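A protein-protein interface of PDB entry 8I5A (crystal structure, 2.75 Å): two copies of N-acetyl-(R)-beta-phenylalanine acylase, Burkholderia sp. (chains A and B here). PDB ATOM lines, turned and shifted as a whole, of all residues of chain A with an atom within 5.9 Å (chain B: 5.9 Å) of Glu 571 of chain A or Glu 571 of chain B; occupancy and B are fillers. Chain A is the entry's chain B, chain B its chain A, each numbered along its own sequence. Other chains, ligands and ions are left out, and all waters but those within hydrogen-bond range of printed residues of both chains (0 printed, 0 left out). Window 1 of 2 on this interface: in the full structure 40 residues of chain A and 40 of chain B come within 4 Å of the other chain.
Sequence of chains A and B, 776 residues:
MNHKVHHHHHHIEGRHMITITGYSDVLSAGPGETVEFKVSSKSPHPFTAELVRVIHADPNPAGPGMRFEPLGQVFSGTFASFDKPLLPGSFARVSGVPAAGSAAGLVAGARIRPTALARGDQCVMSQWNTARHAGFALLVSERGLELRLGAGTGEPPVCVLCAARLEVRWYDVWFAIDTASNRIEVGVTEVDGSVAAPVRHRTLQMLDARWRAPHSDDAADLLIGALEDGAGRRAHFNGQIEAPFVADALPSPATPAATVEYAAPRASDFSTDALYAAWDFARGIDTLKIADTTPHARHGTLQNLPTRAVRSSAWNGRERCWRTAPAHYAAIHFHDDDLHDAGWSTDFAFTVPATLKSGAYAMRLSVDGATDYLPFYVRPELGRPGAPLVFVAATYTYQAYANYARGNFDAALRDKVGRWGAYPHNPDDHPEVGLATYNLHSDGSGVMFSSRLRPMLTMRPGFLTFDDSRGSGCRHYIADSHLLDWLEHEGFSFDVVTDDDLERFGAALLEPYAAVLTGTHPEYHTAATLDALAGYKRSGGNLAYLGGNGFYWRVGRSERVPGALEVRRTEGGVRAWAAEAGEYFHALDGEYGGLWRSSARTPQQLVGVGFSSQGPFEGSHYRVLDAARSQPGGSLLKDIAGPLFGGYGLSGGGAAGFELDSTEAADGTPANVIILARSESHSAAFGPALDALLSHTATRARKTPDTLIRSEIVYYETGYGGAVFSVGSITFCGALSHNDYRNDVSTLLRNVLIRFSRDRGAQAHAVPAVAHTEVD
OE1 of Glu 571 of chain B touches CA of Glu 571 of chain A, 3.1 Å away. Tyr 592 of chain A touches Arg 320 of chain B.
Glu 571 of chain B touches two residues of chain A. Of the printed residues of chain A, Arg 700 of chain B touches Arg 575. Printed residues of chain B within 4 Å of Arg 700 of chain A: Arg 575 (3.5 Å). The nearest residue of chain B that does not touch Glu 571 of chain A is Gly 572 of chain B (4.9 Å). The nearest residue of chain A that does not touch Glu 571 of chain B is Gly 572 of chain A (4.9 Å). The nearest printed residue of chain B that does not touch Tyr 584 of chain A is Tyr 592 of chain B (4.1 Å).
NH1 of Arg 320 of chain B lies within hydrogen-bond range of O of Ser 598 of chain A (3.0 Å). OE1 of Glu 571 of chain A lies within hydrogen-bond range of OH of Tyr 584 of chain B (2.6 Å). The guanidinium group of Arg 575 of chain B lies close to the guanidinium group of Arg 700 of chain A, 3.5 Å away. The side-chain carboxylate of Glu 571 of chain B lies within hydrogen-bond range of the side-chain hydroxyl of Tyr 584 of chain A. The guanidinium group (NH2) of Arg 575 of chain A lies close to the guanidinium group (NH2) of Arg 700 of chain B (3.3 Å).
Of the 13 printed residues of chain B, 5 touch a printed residue of chain A. Along chain B the printed residues that touch a printed residue of chain A span positions 320 to 700. Of the 13 printed residues of chain A, 6 touch a printed residue of chain B. Hydrophobic or aromatic side chains of chain A that line the printed part of chain B: Tyr 584 and Tyr 592. Among the printed residues, 7 pairs touch across the chains.
Glu 571 of chain B touches its own counterpart, Glu 571 of chain A. Glu 571 of chain A touches Tyr 584 of chain B, and with the chains exchanged Tyr 584 of chain A touches Glu 571 of chain B. Arg 575 of chain A touches Arg 700 of chain B, and with the chains exchanged Arg 700 of chain A touches Arg 575 of chain B. Of the 7 pairs that touch across the chains among the printed residues, 5 have their exchanged pair printed and touching as well.
OE2 of Glu 571 of chain B sits at hydrogen-bond distance from OG of Ser 598 of chain B (3.4 Å). The backbone carbonyl oxygen of Arg 569 of chain B is in hydrogen-bond range of the guanidinium group of Arg 575 of chain B, at 2.8 Å. O of Arg 569 of chain A lies within hydrogen-bond range of NH1 of Arg 575 of chain A, at 2.9 Å. The backbone carbonyl oxygen (O) of Glu 571 of chain A lies within hydrogen-bond range of the guanidinium group (NH2) of Arg 575 of chain A (3.3 Å). OG of Ser 598 of chain A lies close to OE2 of Glu 571 of chain A, 3.4 Å away. The side-chain hydroxyl (OH) of Tyr 592 of chain A sits at hydrogen-bond distance from the side-chain carboxylate (OE2) of Glu 571 of chain A (2.5 Å).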
ATOM      1  N   ARG A 569      17.988 -14.804  12.817  1.00  0.00           N
ATOM      2  CA  ARG A 569      18.278 -15.687  11.678  1.00  0.00           C
ATOM      3  C   ARG A 569      19.334 -15.045  10.775  1.00  0.00           C
ATOM      4  O   ARG A 569      19.042 -14.486   9.717  1.00  0.00           O
ATOM      5  CB  ARG A 569      16.988 -16.009  10.931  1.00  0.00           C
ATOM      6  CG  ARG A 569      15.860 -16.440  11.867  1.00  0.00           C
ATOM      7  CD  ARG A 569      14.692 -17.031  11.090  1.00  0.00           C
ATOM      8  NE  ARG A 569      13.630 -17.552  11.942  1.00  0.00           N
ATOM      9  CZ  ARG A 569      13.741 -18.642  12.691  1.00  0.00           C
ATOM     10  NH1 ARG A 569      14.871 -19.333  12.741  1.00  0.00           N
ATOM     11  NH2 ARG A 569      12.693 -19.047  13.413  1.00  0.00           N
ATOM     12  N   THR A 570      20.594 -15.190  11.186  1.00  0.00           N
ATOM     13  CA  THR A 570      21.723 -14.503  10.570  1.00  0.00           C
ATOM     14  C   THR A 570      22.333 -15.321   9.435  1.00  0.00           C
ATOM     15  O   THR A 570      22.235 -16.547   9.394  1.00  0.00           O
ATOM     16  CB  THR A 570      22.808 -14.217  11.608  1.00  0.00           C
ATOM     17  OG1 THR A 570      23.437 -15.446  11.999  1.00  0.00           O
ATOM     18  CG2 THR A 570      22.224 -13.541  12.833  1.00  0.00           C
ATOM     19  N   GLU A 571      22.994 -14.613   8.519  1.00  0.00           N
ATOM     20  CA  GLU A 571      23.892 -15.191   7.507  1.00  0.00           C
ATOM     21  C   GLU A 571      23.178 -15.978   6.408  1.00  0.00           C
ATOM     22  O   GLU A 571      23.213 -15.581   5.243  1.00  0.00           O
ATOM     23  CB  GLU A 571      24.964 -16.068   8.173  1.00  0.00           C
ATOM     24  CG  GLU A 571      25.921 -15.288   9.069  1.00  0.00           C
ATOM     25  CD  GLU A 571      27.198 -16.050   9.375  1.00  0.00           C
ATOM     26  OE1 GLU A 571      27.733 -16.725   8.447  1.00  0.00           O
ATOM     27  OE2 GLU A 571      27.663 -15.967  10.549  1.00  0.00           O
ATOM     28  N   GLY A 572      22.534 -17.086   6.744  1.00  0.00           N
ATOM     29  CA  GLY A 572      21.939 -17.912   5.713  1.00  0.00           C
ATOM     30  C   GLY A 572      21.171 -19.101   6.255  1.00  0.00           C
ATOM     31  O   GLY A 572      20.468 -18.995   7.265  1.00  0.00           O
ATOM     32  N   GLY A 573      21.281 -20.237   5.583  1.00  0.00           N
ATOM     33  CA  GLY A 573      20.498 -21.397   5.941  1.00  0.00           C
ATOM     34  C   GLY A 573      19.080 -21.277   5.436  1.00  0.00           C
ATOM     35  O   GLY A 573      18.687 -20.310   4.764  1.00  0.00           O
ATOM     36  N   ARG A 575      15.697 -20.232   6.167  1.00  0.00           N
ATOM     37  CA  ARG A 575      15.225 -19.307   7.186  1.00  0.00           C
ATOM     38  C   ARG A 575      13.950 -18.595   6.745  1.00  0.00           C
ATOM     39  O   ARG A 575      13.801 -18.237   5.573  1.00  0.00           O
ATOM     40  CB  ARG A 575      16.331 -18.297   7.551  1.00  0.00           C
ATOM     41  CG  ARG A 575      16.902 -17.518   6.399  1.00  0.00           C
ATOM     42  CD  ARG A 575      18.145 -16.773   6.837  1.00  0.00           C
ATOM     43  NE  ARG A 575      18.826 -16.151   5.709  1.00  0.00           N
ATOM     44  CZ  ARG A 575      19.565 -15.056   5.794  1.00  0.00           C
ATOM     45  NH1 ARG A 575      19.717 -14.416   6.945  1.00  0.00           N
ATOM     46  NH2 ARG A 575      20.160 -14.586   4.698  1.00  0.00           N
ATOM     47  N   ALA A 579      17.836 -11.691   9.178  1.00  0.00           N
ATOM     48  CA  ALA A 579      18.284 -10.597  10.021  1.00  0.00           C
ATOM     49  C   ALA A 579      19.010  -9.553   9.181  1.00  0.00           C
ATOM     50  O   ALA A 579      19.517  -9.854   8.104  1.00  0.00           O
ATOM     51  CB  ALA A 579      19.199 -11.135  11.116  1.00  0.00           C
ATOM     52  N   TYR A 584      23.362  -9.012  14.432  1.00  0.00           N
ATOM     53  CA  TYR A 584      23.511 -10.454  14.551  1.00  0.00           C
ATOM     54  C   TYR A 584      23.642 -10.935  15.988  1.00  0.00           C
ATOM     55  O   TYR A 584      23.466 -12.137  16.237  1.00  0.00           O
ATOM     56  CB  TYR A 584      24.730 -10.911  13.753  1.00  0.00           C
ATOM     57  CG  TYR A 584      24.493 -10.969  12.276  1.00  0.00           C
ATOM     58  CD1 TYR A 584      23.318 -10.494  11.705  1.00  0.00           C
ATOM     59  CD2 TYR A 584      25.444 -11.519  11.444  1.00  0.00           C
ATOM     60  CE1 TYR A 584      23.122 -10.556  10.339  1.00  0.00           C
ATOM     61  CE2 TYR A 584      25.253 -11.595  10.095  1.00  0.00           C
ATOM     62  CZ  TYR A 584      24.097 -11.118   9.545  1.00  0.00           C
ATOM     63  OH  TYR A 584      23.959 -11.223   8.187  1.00  0.00           O
ATOM     64  N   TYR A 592      26.534 -14.174  19.644  1.00  0.00           N
ATOM     65  CA  TYR A 592      26.356 -14.242  18.199  1.00  0.00           C
ATOM     66  C   TYR A 592      25.256 -15.241  17.879  1.00  0.00           C
ATOM     67  O   TYR A 592      25.374 -16.430  18.196  1.00  0.00           O
ATOM     68  CB  TYR A 592      27.661 -14.664  17.517  1.00  0.00           C
ATOM     69  CG  TYR A 592      27.661 -14.467  16.012  1.00  0.00           C
ATOM     70  CD1 TYR A 592      27.891 -13.208  15.465  1.00  0.00           C
ATOM     71  CD2 TYR A 592      27.423 -15.530  15.135  1.00  0.00           C
ATOM     72  CE1 TYR A 592      27.879 -12.998  14.096  1.00  0.00           C
ATOM     73  CE2 TYR A 592      27.423 -15.334  13.732  1.00  0.00           C
ATOM     74  CZ  TYR A 592      27.651 -14.052  13.229  1.00  0.00           C
ATOM     75  OH  TYR A 592      27.666 -13.798  11.875  1.00  0.00           O
ATOM     76  N   GLY A 593      24.192 -14.771  17.244  1.00  0.00           N
ATOM     77  CA  GLY A 593      23.059 -15.617  16.961  1.00  0.00           C
ATOM     78  C   GLY A 593      23.118 -16.271  15.602  1.00  0.00           C
ATOM     79  O   GLY A 593      24.043 -16.084  14.807  1.00  0.00           O
ATOM     80  N   LEU A 595      22.653 -19.697  12.941  1.00  0.00           N
ATOM     81  CA  LEU A 595      22.985 -21.107  12.804  1.00  0.00           C
ATOM     82  C   LEU A 595      24.127 -21.491  13.728  1.00  0.00           C
ATOM     83  O   LEU A 595      25.102 -20.750  13.869  1.00  0.00           O
ATOM     84  CB  LEU A 595      23.401 -21.390  11.368  1.00  0.00           C
ATOM     85  CG  LEU A 595      22.366 -21.051  10.308  1.00  0.00           C
ATOM     86  CD1 LEU A 595      23.006 -21.067   8.941  1.00  0.00           C
ATOM     87  CD2 LEU A 595      21.249 -22.061  10.383  1.00  0.00           C
ATOM     88  N   SER A 598      27.357 -21.306  12.202  1.00  0.00           N
ATOM     89  CA  SER A 598      28.001 -20.001  12.225  1.00  0.00           C
ATOM     90  C   SER A 598      28.655 -19.680  13.552  1.00  0.00           C
ATOM     91  O   SER A 598      29.297 -18.624  13.662  1.00  0.00           O
ATOM     92  CB  SER A 598      26.993 -18.930  11.843  1.00  0.00           C
ATOM     93  OG  SER A 598      26.530 -19.218  10.536  1.00  0.00           O
ATOM     94  N   ARG A 700      29.301 -27.710   0.070  1.00  0.00           N
ATOM     95  CA  ARG A 700      30.555 -27.336   0.721  1.00  0.00           C
ATOM     96  C   ARG A 700      31.632 -28.396   0.502  1.00  0.00           C
ATOM     97  O   ARG A 700      32.833 -28.083   0.491  1.00  0.00           O
ATOM     98  CB  ARG A 700      30.323 -27.111   2.223  1.00  0.00           C
ATOM     99  CG  ARG A 700      29.674 -25.772   2.624  1.00  0.00           C
ATOM    100  CD  ARG A 700      29.462 -25.744   4.137  1.00  0.00           C
ATOM    101  NE  ARG A 700      28.940 -24.474   4.633  1.00  0.00           N
ATOM    102  CZ  ARG A 700      29.696 -23.494   5.115  1.00  0.00           C
ATOM    103  NH1 ARG A 700      31.017 -23.612   5.185  1.00  0.00           N
ATOM    104  NH2 ARG A 700      29.118 -22.359   5.520  1.00  0.00           N
ATOM    105  N   ARG B 320      34.373 -12.187  18.006  1.00  0.00           N
ATOM    106  CA  ARG B 320      34.272 -12.384  16.565  1.00  0.00           C
ATOM    107  C   ARG B 320      35.031 -11.341  15.765  1.00  0.00           C
ATOM    108  O   ARG B 320      35.058 -11.437  14.527  1.00  0.00           O
ATOM    109  CB  ARG B 320      32.804 -12.353  16.101  1.00  0.00           C
ATOM    110  CG  ARG B 320      31.854 -13.338  16.746  1.00  0.00           C
ATOM    111  CD  ARG B 320      32.356 -14.766  16.621  1.00  0.00           C
ATOM    112  NE  ARG B 320      31.496 -15.751  17.272  1.00  0.00           N
ATOM    113  CZ  ARG B 320      30.660 -16.546  16.617  1.00  0.00           C
ATOM    114  NH1 ARG B 320      30.514 -16.448  15.300  1.00  0.00           N
ATOM    115  NH2 ARG B 320      29.965 -17.466  17.293  1.00  0.00           N
ATOM    116  N   ARG B 569      35.185 -14.504   1.913  1.00  0.00           N
ATOM    117  CA  ARG B 569      33.889 -14.889   1.369  1.00  0.00           C
ATOM    118  C   ARG B 569      32.999 -15.351   2.517  1.00  0.00           C
ATOM    119  O   ARG B 569      32.880 -16.541   2.821  1.00  0.00           O
ATOM    120  CB  ARG B 569      34.070 -15.950   0.295  1.00  0.00           C
ATOM    121  CG  ARG B 569      35.098 -15.536  -0.726  1.00  0.00           C
ATOM    122  CD  ARG B 569      35.039 -16.369  -1.997  1.00  0.00           C
ATOM    123  NE  ARG B 569      36.027 -15.927  -2.973  1.00  0.00           N
ATOM    124  CZ  ARG B 569      35.870 -14.886  -3.778  1.00  0.00           C
ATOM    125  NH1 ARG B 569      34.772 -14.142  -3.736  1.00  0.00           N
ATOM    126  NH2 ARG B 569      36.833 -14.589  -4.656  1.00  0.00           N
ATOM    127  N   THR B 570      32.373 -14.374   3.170  1.00  0.00           N
ATOM    128  CA  THR B 570      31.625 -14.609   4.393  1.00  0.00           C
ATOM    129  C   THR B 570      30.153 -14.896   4.100  1.00  0.00           C
ATOM    130  O   THR B 570      29.615 -14.528   3.055  1.00  0.00           O
ATOM    131  CB  THR B 570      31.720 -13.399   5.340  1.00  0.00           C
ATOM    132  OG1 THR B 570      30.961 -12.307   4.801  1.00  0.00           O
ATOM    133  CG2 THR B 570      33.171 -12.958   5.558  1.00  0.00           C
ATOM    134  N   GLU B 571      29.510 -15.561   5.065  1.00  0.00           N
ATOM    135  CA  GLU B 571      28.056 -15.671   5.194  1.00  0.00           C
ATOM    136  C   GLU B 571      27.412 -16.549   4.123  1.00  0.00           C
ATOM    137  O   GLU B 571      26.830 -17.587   4.442  1.00  0.00           O
ATOM    138  CB  GLU B 571      27.405 -14.276   5.190  1.00  0.00           C
ATOM    139  CG  GLU B 571      27.740 -13.413   6.396  1.00  0.00           C
ATOM    140  CD  GLU B 571      26.683 -12.361   6.734  1.00  0.00           C
ATOM    141  OE1 GLU B 571      25.464 -12.627   6.596  1.00  0.00           O
ATOM    142  OE2 GLU B 571      27.079 -11.250   7.160  1.00  0.00           O
ATOM    143  N   GLY B 572      27.467 -16.140   2.862  1.00  0.00           N
ATOM    144  CA  GLY B 572      26.759 -16.885   1.844  1.00  0.00           C
ATOM    145  C   GLY B 572      26.950 -16.336   0.453  1.00  0.00           C
ATOM    146  O   GLY B 572      28.021 -15.805   0.133  1.00  0.00           O
ATOM    147  N   GLY B 573      25.906 -16.416  -0.374  1.00  0.00           N
ATOM    148  CA  GLY B 573      26.047 -16.086  -1.777  1.00  0.00           C
ATOM    149  C   GLY B 573      26.702 -17.199  -2.592  1.00  0.00           C
ATOM    150  O   GLY B 573      26.978 -18.320  -2.128  1.00  0.00           O
ATOM    151  N   ARG B 575      29.798 -18.569  -3.917  1.00  0.00           N
ATOM    152  CA  ARG B 575      31.189 -18.387  -3.524  1.00  0.00           C
ATOM    153  C   ARG B 575      32.027 -19.633  -3.803  1.00  0.00           C
ATOM    154  O   ARG B 575      31.548 -20.765  -3.666  1.00  0.00           O
ATOM    155  CB  ARG B 575      31.303 -18.004  -2.039  1.00  0.00           C
ATOM    156  CG  ARG B 575      30.177 -18.496  -1.153  1.00  0.00           C
ATOM    157  CD  ARG B 575      30.444 -18.130   0.294  1.00  0.00           C
ATOM    158  NE  ARG B 575      29.701 -19.019   1.172  1.00  0.00           N
ATOM    159  CZ  ARG B 575      29.749 -18.975   2.496  1.00  0.00           C
ATOM    160  NH1 ARG B 575      30.533 -18.117   3.126  1.00  0.00           N
ATOM    161  NH2 ARG B 575      28.977 -19.798   3.205  1.00  0.00           N
ATOM    162  N   ALA B 579      34.511 -18.606   4.247  1.00  0.00           N
ATOM    163  CA  ALA B 579      35.282 -18.217   5.424  1.00  0.00           C
ATOM    164  C   ALA B 579      34.814 -18.966   6.674  1.00  0.00           C
ATOM    165  O   ALA B 579      33.641 -19.319   6.803  1.00  0.00           O
ATOM    166  CB  ALA B 579      35.145 -16.713   5.654  1.00  0.00           C
ATOM    167  N   TYR B 584      35.644 -13.037   9.820  1.00  0.00           N
ATOM    168  CA  TYR B 584      34.923 -12.261   8.822  1.00  0.00           C
ATOM    169  C   TYR B 584      35.527 -10.874   8.585  1.00  0.00           C
ATOM    170  O   TYR B 584      35.270 -10.260   7.537  1.00  0.00           O
ATOM    171  CB  TYR B 584      33.452 -12.134   9.247  1.00  0.00           C
ATOM    172  CG  TYR B 584      32.637 -13.390   8.993  1.00  0.00           C
ATOM    173  CD1 TYR B 584      33.260 -14.613   8.717  1.00  0.00           C
ATOM    174  CD2 TYR B 584      31.249 -13.353   9.010  1.00  0.00           C
ATOM    175  CE1 TYR B 584      32.507 -15.756   8.466  1.00  0.00           C
ATOM    176  CE2 TYR B 584      30.498 -14.483   8.761  1.00  0.00           C
ATOM    177  CZ  TYR B 584      31.130 -15.677   8.485  1.00  0.00           C
ATOM    178  OH  TYR B 584      30.369 -16.790   8.246  1.00  0.00           O
ATOM    179  N   TYR B 592      34.536  -5.393   7.956  1.00  0.00           N
ATOM    180  CA  TYR B 592      33.713  -6.578   7.728  1.00  0.00           C
ATOM    181  C   TYR B 592      33.678  -6.915   6.238  1.00  0.00           C
ATOM    182  O   TYR B 592      33.197  -6.114   5.429  1.00  0.00           O
ATOM    183  CB  TYR B 592      32.302  -6.328   8.252  1.00  0.00           C
ATOM    184  CG  TYR B 592      31.455  -7.557   8.371  1.00  0.00           C
ATOM    185  CD1 TYR B 592      31.503  -8.344   9.516  1.00  0.00           C
ATOM    186  CD2 TYR B 592      30.597  -7.939   7.340  1.00  0.00           C
ATOM    187  CE1 TYR B 592      30.728  -9.493   9.621  1.00  0.00           C
ATOM    188  CE2 TYR B 592      29.802  -9.100   7.439  1.00  0.00           C
ATOM    189  CZ  TYR B 592      29.873  -9.865   8.580  1.00  0.00           C
ATOM    190  OH  TYR B 592      29.098 -10.996   8.702  1.00  0.00           O
ATOM    191  N   GLY B 593      34.183  -8.101   5.865  1.00  0.00           N
ATOM    192  CA  GLY B 593      34.252  -8.501   4.475  1.00  0.00           C
ATOM    193  C   GLY B 593      33.051  -9.316   4.020  1.00  0.00           C
ATOM    194  O   GLY B 593      32.155  -9.660   4.792  1.00  0.00           O
ATOM    195  N   SER B 598      25.952  -7.785   2.831  1.00  0.00           N
ATOM    196  CA  SER B 598      26.262  -8.026   4.236  1.00  0.00           C
ATOM    197  C   SER B 598      26.794  -6.798   4.960  1.00  0.00           C
ATOM    198  O   SER B 598      26.980  -6.861   6.186  1.00  0.00           O
ATOM    199  CB  SER B 598      27.270  -9.164   4.353  1.00  0.00           C
ATOM    200  OG  SER B 598      26.694 -10.374   3.910  1.00  0.00           O
ATOM    201  N   ARG B 700      13.940 -13.785  -1.273  1.00  0.00           N
ATOM    202  CA  ARG B 700      13.800 -12.811  -0.197  1.00  0.00           C
ATOM    203  C   ARG B 700      12.517 -12.000  -0.348  1.00  0.00           C
ATOM    204  O   ARG B 700      11.979 -11.481   0.640  1.00  0.00           O
ATOM    205  CB  ARG B 700      15.012 -11.881  -0.176  1.00  0.00           C
ATOM    206  CG  ARG B 700      16.210 -12.359   0.632  1.00  0.00           C
ATOM    207  CD  ARG B 700      17.410 -11.513   0.284  1.00  0.00           C
ATOM    208  NE  ARG B 700      18.601 -11.900   1.023  1.00  0.00           N
ATOM    209  CZ  ARG B 700      18.883 -11.492   2.254  1.00  0.00           C
ATOM    210  NH1 ARG B 700      18.068 -10.681   2.911  1.00  0.00           N
ATOM    211  NH2 ARG B 700      20.011 -11.909   2.836  1.00  0.00           N
